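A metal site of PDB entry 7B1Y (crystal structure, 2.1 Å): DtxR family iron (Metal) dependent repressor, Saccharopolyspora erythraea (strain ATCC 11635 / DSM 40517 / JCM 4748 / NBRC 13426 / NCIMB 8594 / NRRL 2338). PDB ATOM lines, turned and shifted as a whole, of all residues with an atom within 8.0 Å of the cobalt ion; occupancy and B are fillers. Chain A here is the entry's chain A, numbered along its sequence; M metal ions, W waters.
The guanidinium group (NH1) of Arg 15 is in salt-bridge range of the side-chain carboxylate (OE1) of Glu 107, at 3.3 Å. The backbone carbonyl oxygen of Met 12 lies within hydrogen-bond range of the side-chain hydroxyl of Thr 16, 2.6 Å away. The side-chain carboxylate of Glu 107 sits at hydrogen-bond distance from a ring nitrogen (ND1) of His 81 (3.0 Å). OD1 of CSD 104 is in hydrogen-bond range of NE2 of His 100 (3.3 Å). OD1 of CSD 104 is in salt-bridge range of the guanidinium group (NH1) of Arg 15. OE1 of Glu 11 lies within hydrogen-bond range of ND1 of His 108.
The cobalt ion is bound by OE2 of Glu 107 (2.0 Å), O of CSD 104 (2.1 Å), NE2 of His 108 (2.2 Å), OD2 of CSD 104 (2.3 Å), SD of Met 12 (2.4 Å) and water W1 (2.5 Å). The cobalt ion has six donor atoms within binding distance.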
ATOM      1  N   ASP A   5      30.090  22.741  21.660  1.00  0.00           N
ATOM      2  CA  ASP A   5      29.397  21.421  21.646  1.00  0.00           C
ATOM      3  C   ASP A   5      28.923  21.088  23.071  1.00  0.00           C
ATOM      4  O   ASP A   5      27.689  21.130  23.287  1.00  0.00           O
ATOM      5  CB  ASP A   5      30.308  20.335  21.055  1.00  0.00           C
ATOM      6  CG  ASP A   5      29.615  19.013  20.746  1.00  0.00           C
ATOM      7  OD1 ASP A   5      28.371  18.946  20.897  1.00  0.00           O
ATOM      8  OD2 ASP A   5      30.322  18.059  20.354  1.00  0.00           O
ATOM      9  N   LEU A   6      29.843  20.800  23.988  1.00  0.00           N
ATOM     10  CA  LEU A   6      29.557  20.481  25.416  1.00  0.00           C
ATOM     11  C   LEU A   6      29.315  21.780  26.198  1.00  0.00           C
ATOM     12  O   LEU A   6      28.717  21.695  27.293  1.00  0.00           O
ATOM     13  CB  LEU A   6      30.726  19.699  26.020  1.00  0.00           C
ATOM     14  CG  LEU A   6      30.954  18.292  25.478  1.00  0.00           C
ATOM     15  CD1 LEU A   6      32.071  17.604  26.239  1.00  0.00           C
ATOM     16  CD2 LEU A   6      29.687  17.453  25.532  1.00  0.00           C
ATOM     17  N   ILE A   7      29.787  22.923  25.676  1.00  0.00           N
ATOM     18  CA  ILE A   7      29.690  24.275  26.308  1.00  0.00           C
ATOM     19  C   ILE A   7      30.699  24.354  27.461  1.00  0.00           C
ATOM     20  O   ILE A   7      31.580  25.240  27.419  1.00  0.00           O
ATOM     21  CB  ILE A   7      28.257  24.620  26.762  1.00  0.00           C
ATOM     22  CG1 ILE A   7      27.209  24.293  25.696  1.00  0.00           C
ATOM     23  CG2 ILE A   7      28.156  26.062  27.209  1.00  0.00           C
ATOM     24  CD1 ILE A   7      27.420  25.015  24.376  1.00  0.00           C
ATOM     25  N   ASP A   8      30.571  23.468  28.462  1.00  0.00           N
ATOM     26  CA  ASP A   8      31.496  23.350  29.615  1.00  0.00           C
ATOM     27  C   ASP A   8      31.856  21.864  29.805  1.00  0.00           C
ATOM     28  O   ASP A   8      30.977  21.097  30.239  1.00  0.00           O
ATOM     29  CB  ASP A   8      30.876  23.963  30.876  1.00  0.00           C
ATOM     30  CG  ASP A   8      31.860  24.174  32.018  1.00  0.00           C
ATOM     31  OD1 ASP A   8      32.524  23.191  32.413  1.00  0.00           O
ATOM     32  OD2 ASP A   8      31.958  25.314  32.500  1.00  0.00           O
ATOM     33  N   GLU A  11      31.655  20.507  33.666  1.00  0.00           N
ATOM     34  CA  GLU A  11      30.259  20.382  34.161  1.00  0.00           C
ATOM     35  C   GLU A  11      29.604  19.152  33.532  1.00  0.00           C
ATOM     36  O   GLU A  11      28.857  18.452  34.250  1.00  0.00           O
ATOM     37  CB  GLU A  11      29.471  21.667  33.904  1.00  0.00           C
ATOM     38  CG  GLU A  11      29.925  22.831  34.757  1.00  0.00           C
ATOM     39  CD  GLU A  11      29.090  24.101  34.686  1.00  0.00           C
ATOM     40  OE1 GLU A  11      28.213  24.178  33.798  1.00  0.00           O
ATOM     41  OE2 GLU A  11      29.312  24.995  35.520  1.00  0.00           O
ATOM     42  N   MET A  12      29.877  18.870  32.255  1.00  0.00           N
ATOM     43  CA  MET A  12      29.285  17.743  31.493  1.00  0.00           C
ATOM     44  C   MET A  12      29.860  16.409  31.983  1.00  0.00           C
ATOM     45  O   MET A  12      29.092  15.434  32.014  1.00  0.00           O
ATOM     46  CB  MET A  12      29.522  17.879  29.983  1.00  0.00           C
ATOM     47  CG  MET A  12      28.581  18.846  29.296  1.00  0.00           C
ATOM     48  SD  MET A  12      26.845  18.610  29.774  1.00  0.00           S
ATOM     49  CE  MET A  12      26.545  16.944  29.201  1.00  0.00           C
ATOM     50  N   TYR A  13      31.146  16.375  32.347  1.00  0.00           N
ATOM     51  CA  TYR A  13      31.805  15.189  32.960  1.00  0.00           C
ATOM     52  C   TYR A  13      31.181  14.913  34.331  1.00  0.00           C
ATOM     53  O   TYR A  13      30.888  13.748  34.640  1.00  0.00           O
ATOM     54  CB  TYR A  13      33.318  15.388  33.072  1.00  0.00           C
ATOM     55  CG  TYR A  13      34.096  14.954  31.851  1.00  0.00           C
ATOM     56  CD1 TYR A  13      33.797  15.463  30.592  1.00  0.00           C
ATOM     57  CD2 TYR A  13      35.149  14.070  31.952  1.00  0.00           C
ATOM     58  CE1 TYR A  13      34.511  15.080  29.471  1.00  0.00           C
ATOM     59  CE2 TYR A  13      35.872  13.670  30.833  1.00  0.00           C
ATOM     60  CZ  TYR A  13      35.561  14.184  29.592  1.00  0.00           C
ATOM     61  OH  TYR A  13      36.275  13.803  28.494  1.00  0.00           O
ATOM     62  N   ARG A  15      28.163  15.920  35.490  1.00  0.00           N
ATOM     63  CA  ARG A  15      26.728  15.567  35.331  1.00  0.00           C
ATOM     64  C   ARG A  15      26.612  14.147  34.754  1.00  0.00           C
ATOM     65  O   ARG A  15      25.682  13.433  35.163  1.00  0.00           O
ATOM     66  CB  ARG A  15      25.981  16.587  34.448  1.00  0.00           C
ATOM     67  CG  ARG A  15      24.530  16.787  34.839  1.00  0.00           C
ATOM     68  CD  ARG A  15      23.654  17.129  33.654  1.00  0.00           C
ATOM     69  NE  ARG A  15      23.332  15.954  32.865  1.00  0.00           N
ATOM     70  CZ  ARG A  15      22.959  15.947  31.593  1.00  0.00           C
ATOM     71  NH1 ARG A  15      22.839  17.082  30.912  1.00  0.00           N
ATOM     72  NH2 ARG A  15      22.694  14.798  30.986  1.00  0.00           N
ATOM     73  N   THR A  16      27.532  13.765  33.861  1.00  0.00           N
ATOM     74  CA  THR A  16      27.588  12.415  33.235  1.00  0.00           C
ATOM     75  C   THR A  16      27.851  11.357  34.316  1.00  0.00           C
ATOM     76  O   THR A  16      27.239  10.274  34.242  1.00  0.00           O
ATOM     77  CB  THR A  16      28.635  12.341  32.116  1.00  0.00           C
ATOM     78  OG1 THR A  16      28.219  13.225  31.075  1.00  0.00           O
ATOM     79  CG2 THR A  16      28.801  10.948  31.561  1.00  0.00           C
ATOM     80  N   LEU A  36      29.549  10.882  25.833  1.00  0.00           N
ATOM     81  CA  LEU A  36      29.966  12.220  25.319  1.00  0.00           C
ATOM     82  C   LEU A  36      30.662  12.075  23.966  1.00  0.00           C
ATOM     83  O   LEU A  36      31.075  13.109  23.402  1.00  0.00           O
ATOM     84  CB  LEU A  36      30.870  12.900  26.359  1.00  0.00           C
ATOM     85  CG  LEU A  36      30.260  13.089  27.743  1.00  0.00           C
ATOM     86  CD1 LEU A  36      31.202  13.870  28.651  1.00  0.00           C
ATOM     87  CD2 LEU A  36      28.912  13.775  27.674  1.00  0.00           C
ATOM     88  N   VAL A  77      24.535  21.843  38.600  1.00  0.00           N
ATOM     89  CA  VAL A  77      24.307  21.753  37.123  1.00  0.00           C
ATOM     90  C   VAL A  77      22.997  20.989  36.864  1.00  0.00           C
ATOM     91  O   VAL A  77      22.252  21.407  35.953  1.00  0.00           O
ATOM     92  CB  VAL A  77      25.507  21.091  36.402  1.00  0.00           C
ATOM     93  CG1 VAL A  77      25.207  20.821  34.932  1.00  0.00           C
ATOM     94  CG2 VAL A  77      26.770  21.927  36.532  1.00  0.00           C
ATOM     95  N   HIS A  81      19.570  22.308  35.133  1.00  0.00           N
ATOM     96  CA  HIS A  81      19.073  21.456  34.017  1.00  0.00           C
ATOM     97  C   HIS A  81      17.564  21.226  34.152  1.00  0.00           C
ATOM     98  O   HIS A  81      16.822  21.543  33.193  1.00  0.00           O
ATOM     99  CB  HIS A  81      19.846  20.139  33.967  1.00  0.00           C
ATOM    100  CG  HIS A  81      19.421  19.233  32.860  1.00  0.00           C
ATOM    101  ND1 HIS A  81      19.905  19.378  31.585  1.00  0.00           N
ATOM    102  CD2 HIS A  81      18.543  18.212  32.839  1.00  0.00           C
ATOM    103  CE1 HIS A  81      19.347  18.457  30.815  1.00  0.00           C
ATOM    104  NE2 HIS A  81      18.512  17.737  31.559  1.00  0.00           N
ATOM    105  N   HIS A 100      15.198  18.426  26.559  1.00  0.00           N
ATOM    106  CA  HIS A 100      16.456  17.992  27.244  1.00  0.00           C
ATOM    107  C   HIS A 100      17.672  18.565  26.526  1.00  0.00           C
ATOM    108  O   HIS A 100      18.564  19.100  27.221  1.00  0.00           O
ATOM    109  CB  HIS A 100      16.508  16.463  27.354  1.00  0.00           C
ATOM    110  CG  HIS A 100      17.844  15.967  27.798  1.00  0.00           C
ATOM    111  ND1 HIS A 100      18.211  15.929  29.126  1.00  0.00           N
ATOM    112  CD2 HIS A 100      18.902  15.516  27.094  1.00  0.00           C
ATOM    113  CE1 HIS A 100      19.443  15.466  29.226  1.00  0.00           C
ATOM    114  NE2 HIS A 100      19.880  15.200  27.998  1.00  0.00           N
ATOM    115  N   LEU A 101      17.722  18.461  25.195  1.00  0.00           N
ATOM    116  CA  LEU A 101      18.853  18.929  24.338  1.00  0.00           C
ATOM    117  C   LEU A 101      19.050  20.439  24.536  1.00  0.00           C
ATOM    118  O   LEU A 101      20.207  20.891  24.486  1.00  0.00           O
ATOM    119  CB  LEU A 101      18.566  18.610  22.867  1.00  0.00           C
ATOM    120  CG  LEU A 101      18.975  17.207  22.401  1.00  0.00           C
ATOM    121  CD1 LEU A 101      18.062  16.141  22.992  1.00  0.00           C
ATOM    122  CD2 LEU A 101      18.971  17.123  20.887  1.00  0.00           C
ATOM    123  N   GLU A 102      17.956  21.183  24.735  1.00  0.00           N
ATOM    124  CA  GLU A 102      17.969  22.640  25.013  1.00  0.00           C
ATOM    125  C   GLU A 102      18.514  22.871  26.424  1.00  0.00           C
ATOM    126  O   GLU A 102      19.473  23.669  26.565  1.00  0.00           O
ATOM    127  CB  GLU A 102      16.565  23.239  24.874  1.00  0.00           C
ATOM    128  CG  GLU A 102      16.555  24.746  24.799  1.00  0.00           C
ATOM    129  CD  GLU A 102      17.048  25.339  23.489  1.00  0.00           C
ATOM    130  OE1 GLU A 102      16.916  24.658  22.452  1.00  0.00           O
ATOM    131  OE2 GLU A 102      17.547  26.486  23.504  1.00  0.00           O
ATOM    132  N   ALA A 103      17.946  22.194  27.428  1.00  0.00           N
ATOM    133  CA  ALA A 103      18.300  22.299  28.860  1.00  0.00           C
ATOM    134  C   ALA A 103      19.738  21.843  29.080  1.00  0.00           C
ATOM    135  O   ALA A 103      20.365  22.229  30.068  1.00  0.00           O
ATOM    136  CB  ALA A 103      17.334  21.509  29.692  1.00  0.00           C
ATOM    137  N   CSD A 104      20.256  21.008  28.179  1.00  0.00           N
ATOM    138  CA  CSD A 104      21.619  20.497  28.260  1.00  0.00           C
ATOM    139  CB  CSD A 104      21.850  19.360  27.259  1.00  0.00           C
ATOM    140  SG  CSD A 104      22.960  18.132  27.998  1.00  0.00           S
ATOM    141  C   CSD A 104      22.631  21.627  28.026  1.00  0.00           C
ATOM    142  O   CSD A 104      23.761  21.531  28.470  1.00  0.00           O
ATOM    143  OD1 CSD A 104      22.688  16.853  27.290  1.00  0.00           O
ATOM    144  OD2 CSD A 104      24.466  18.564  27.684  1.00  0.00           O
ATOM    145  N   ARG A 105      22.205  22.678  27.303  1.00  0.00           N
ATOM    146  CA  ARG A 105      23.060  23.831  27.062  1.00  0.00           C
ATOM    147  C   ARG A 105      22.771  24.919  28.108  1.00  0.00           C
ATOM    148  O   ARG A 105      23.731  25.554  28.563  1.00  0.00           O
ATOM    149  CB  ARG A 105      22.830  24.355  25.648  1.00  0.00           C
ATOM    150  CG  ARG A 105      23.369  23.454  24.549  1.00  0.00           C
ATOM    151  CD  ARG A 105      23.420  24.174  23.207  1.00  0.00           C
ATOM    152  NE  ARG A 105      22.125  24.762  22.859  1.00  0.00           N
ATOM    153  CZ  ARG A 105      21.088  24.088  22.378  1.00  0.00           C
ATOM    154  NH1 ARG A 105      21.165  22.789  22.151  1.00  0.00           N
ATOM    155  NH2 ARG A 105      19.961  24.727  22.108  1.00  0.00           N
ATOM    156  N   TRP A 106      21.491  25.111  28.460  1.00  0.00           N
ATOM    157  CA  TRP A 106      21.013  26.148  29.420  1.00  0.00           C
ATOM    158  C   TRP A 106      21.613  25.926  30.816  1.00  0.00           C
ATOM    159  O   TRP A 106      21.861  26.926  31.514  1.00  0.00           O
ATOM    160  CB  TRP A 106      19.481  26.169  29.466  1.00  0.00           C
ATOM    161  CG  TRP A 106      18.831  26.845  28.295  1.00  0.00           C
ATOM    162  CD1 TRP A 106      19.263  26.851  26.998  1.00  0.00           C
ATOM    163  CD2 TRP A 106      17.614  27.599  28.313  1.00  0.00           C
ATOM    164  NE1 TRP A 106      18.413  27.569  26.211  1.00  0.00           N
ATOM    165  CE2 TRP A 106      17.389  28.041  26.998  1.00  0.00           C
ATOM    166  CE3 TRP A 106      16.702  27.956  29.314  1.00  0.00           C
ATOM    167  CZ2 TRP A 106      16.280  28.819  26.648  1.00  0.00           C
ATOM    168  CZ3 TRP A 106      15.605  28.730  28.969  1.00  0.00           C
ATOM    169  CH2 TRP A 106      15.401  29.149  27.659  1.00  0.00           C
ATOM    170  N   GLU A 107      21.824  24.665  31.198  1.00  0.00           N
ATOM    171  CA  GLU A 107      22.314  24.254  32.541  1.00  0.00           C
ATOM    172  C   GLU A 107      23.666  24.909  32.877  1.00  0.00           C
ATOM    173  O   GLU A 107      24.002  24.972  34.066  1.00  0.00           O
ATOM    174  CB  GLU A 107      22.416  22.727  32.650  1.00  0.00           C
ATOM    175  CG  GLU A 107      23.433  22.100  31.716  1.00  0.00           C
ATOM    176  CD  GLU A 107      23.462  20.577  31.719  1.00  0.00           C
ATOM    177  OE1 GLU A 107      22.697  19.972  32.499  1.00  0.00           O
ATOM    178  OE2 GLU A 107      24.249  19.991  30.958  1.00  0.00           O
ATOM    179  N   HIS A 108      24.404  25.389  31.858  1.00  0.00           N
ATOM    180  CA  HIS A 108      25.789  25.906  32.000  1.00  0.00           C
ATOM    181  C   HIS A 108      25.825  27.435  32.157  1.00  0.00           C
ATOM    182  O   HIS A 108      26.889  27.939  32.536  1.00  0.00           O
ATOM    183  CB  HIS A 108      26.650  25.448  30.809  1.00  0.00           C
ATOM    184  CG  HIS A 108      26.632  23.970  30.613  1.00  0.00           C
ATOM    185  ND1 HIS A 108      27.235  23.103  31.505  1.00  0.00           N
ATOM    186  CD2 HIS A 108      26.091  23.204  29.645  1.00  0.00           C
ATOM    187  CE1 HIS A 108      27.064  21.864  31.097  1.00  0.00           C
ATOM    188  NE2 HIS A 108      26.359  21.901  29.957  1.00  0.00           N
HETATM  189 CO    CO M   1      25.164  20.201  29.194  1.00  0.00          CO
HETATM  190  O   HOH W   1      26.194  20.514  26.990  1.00  0.00           O
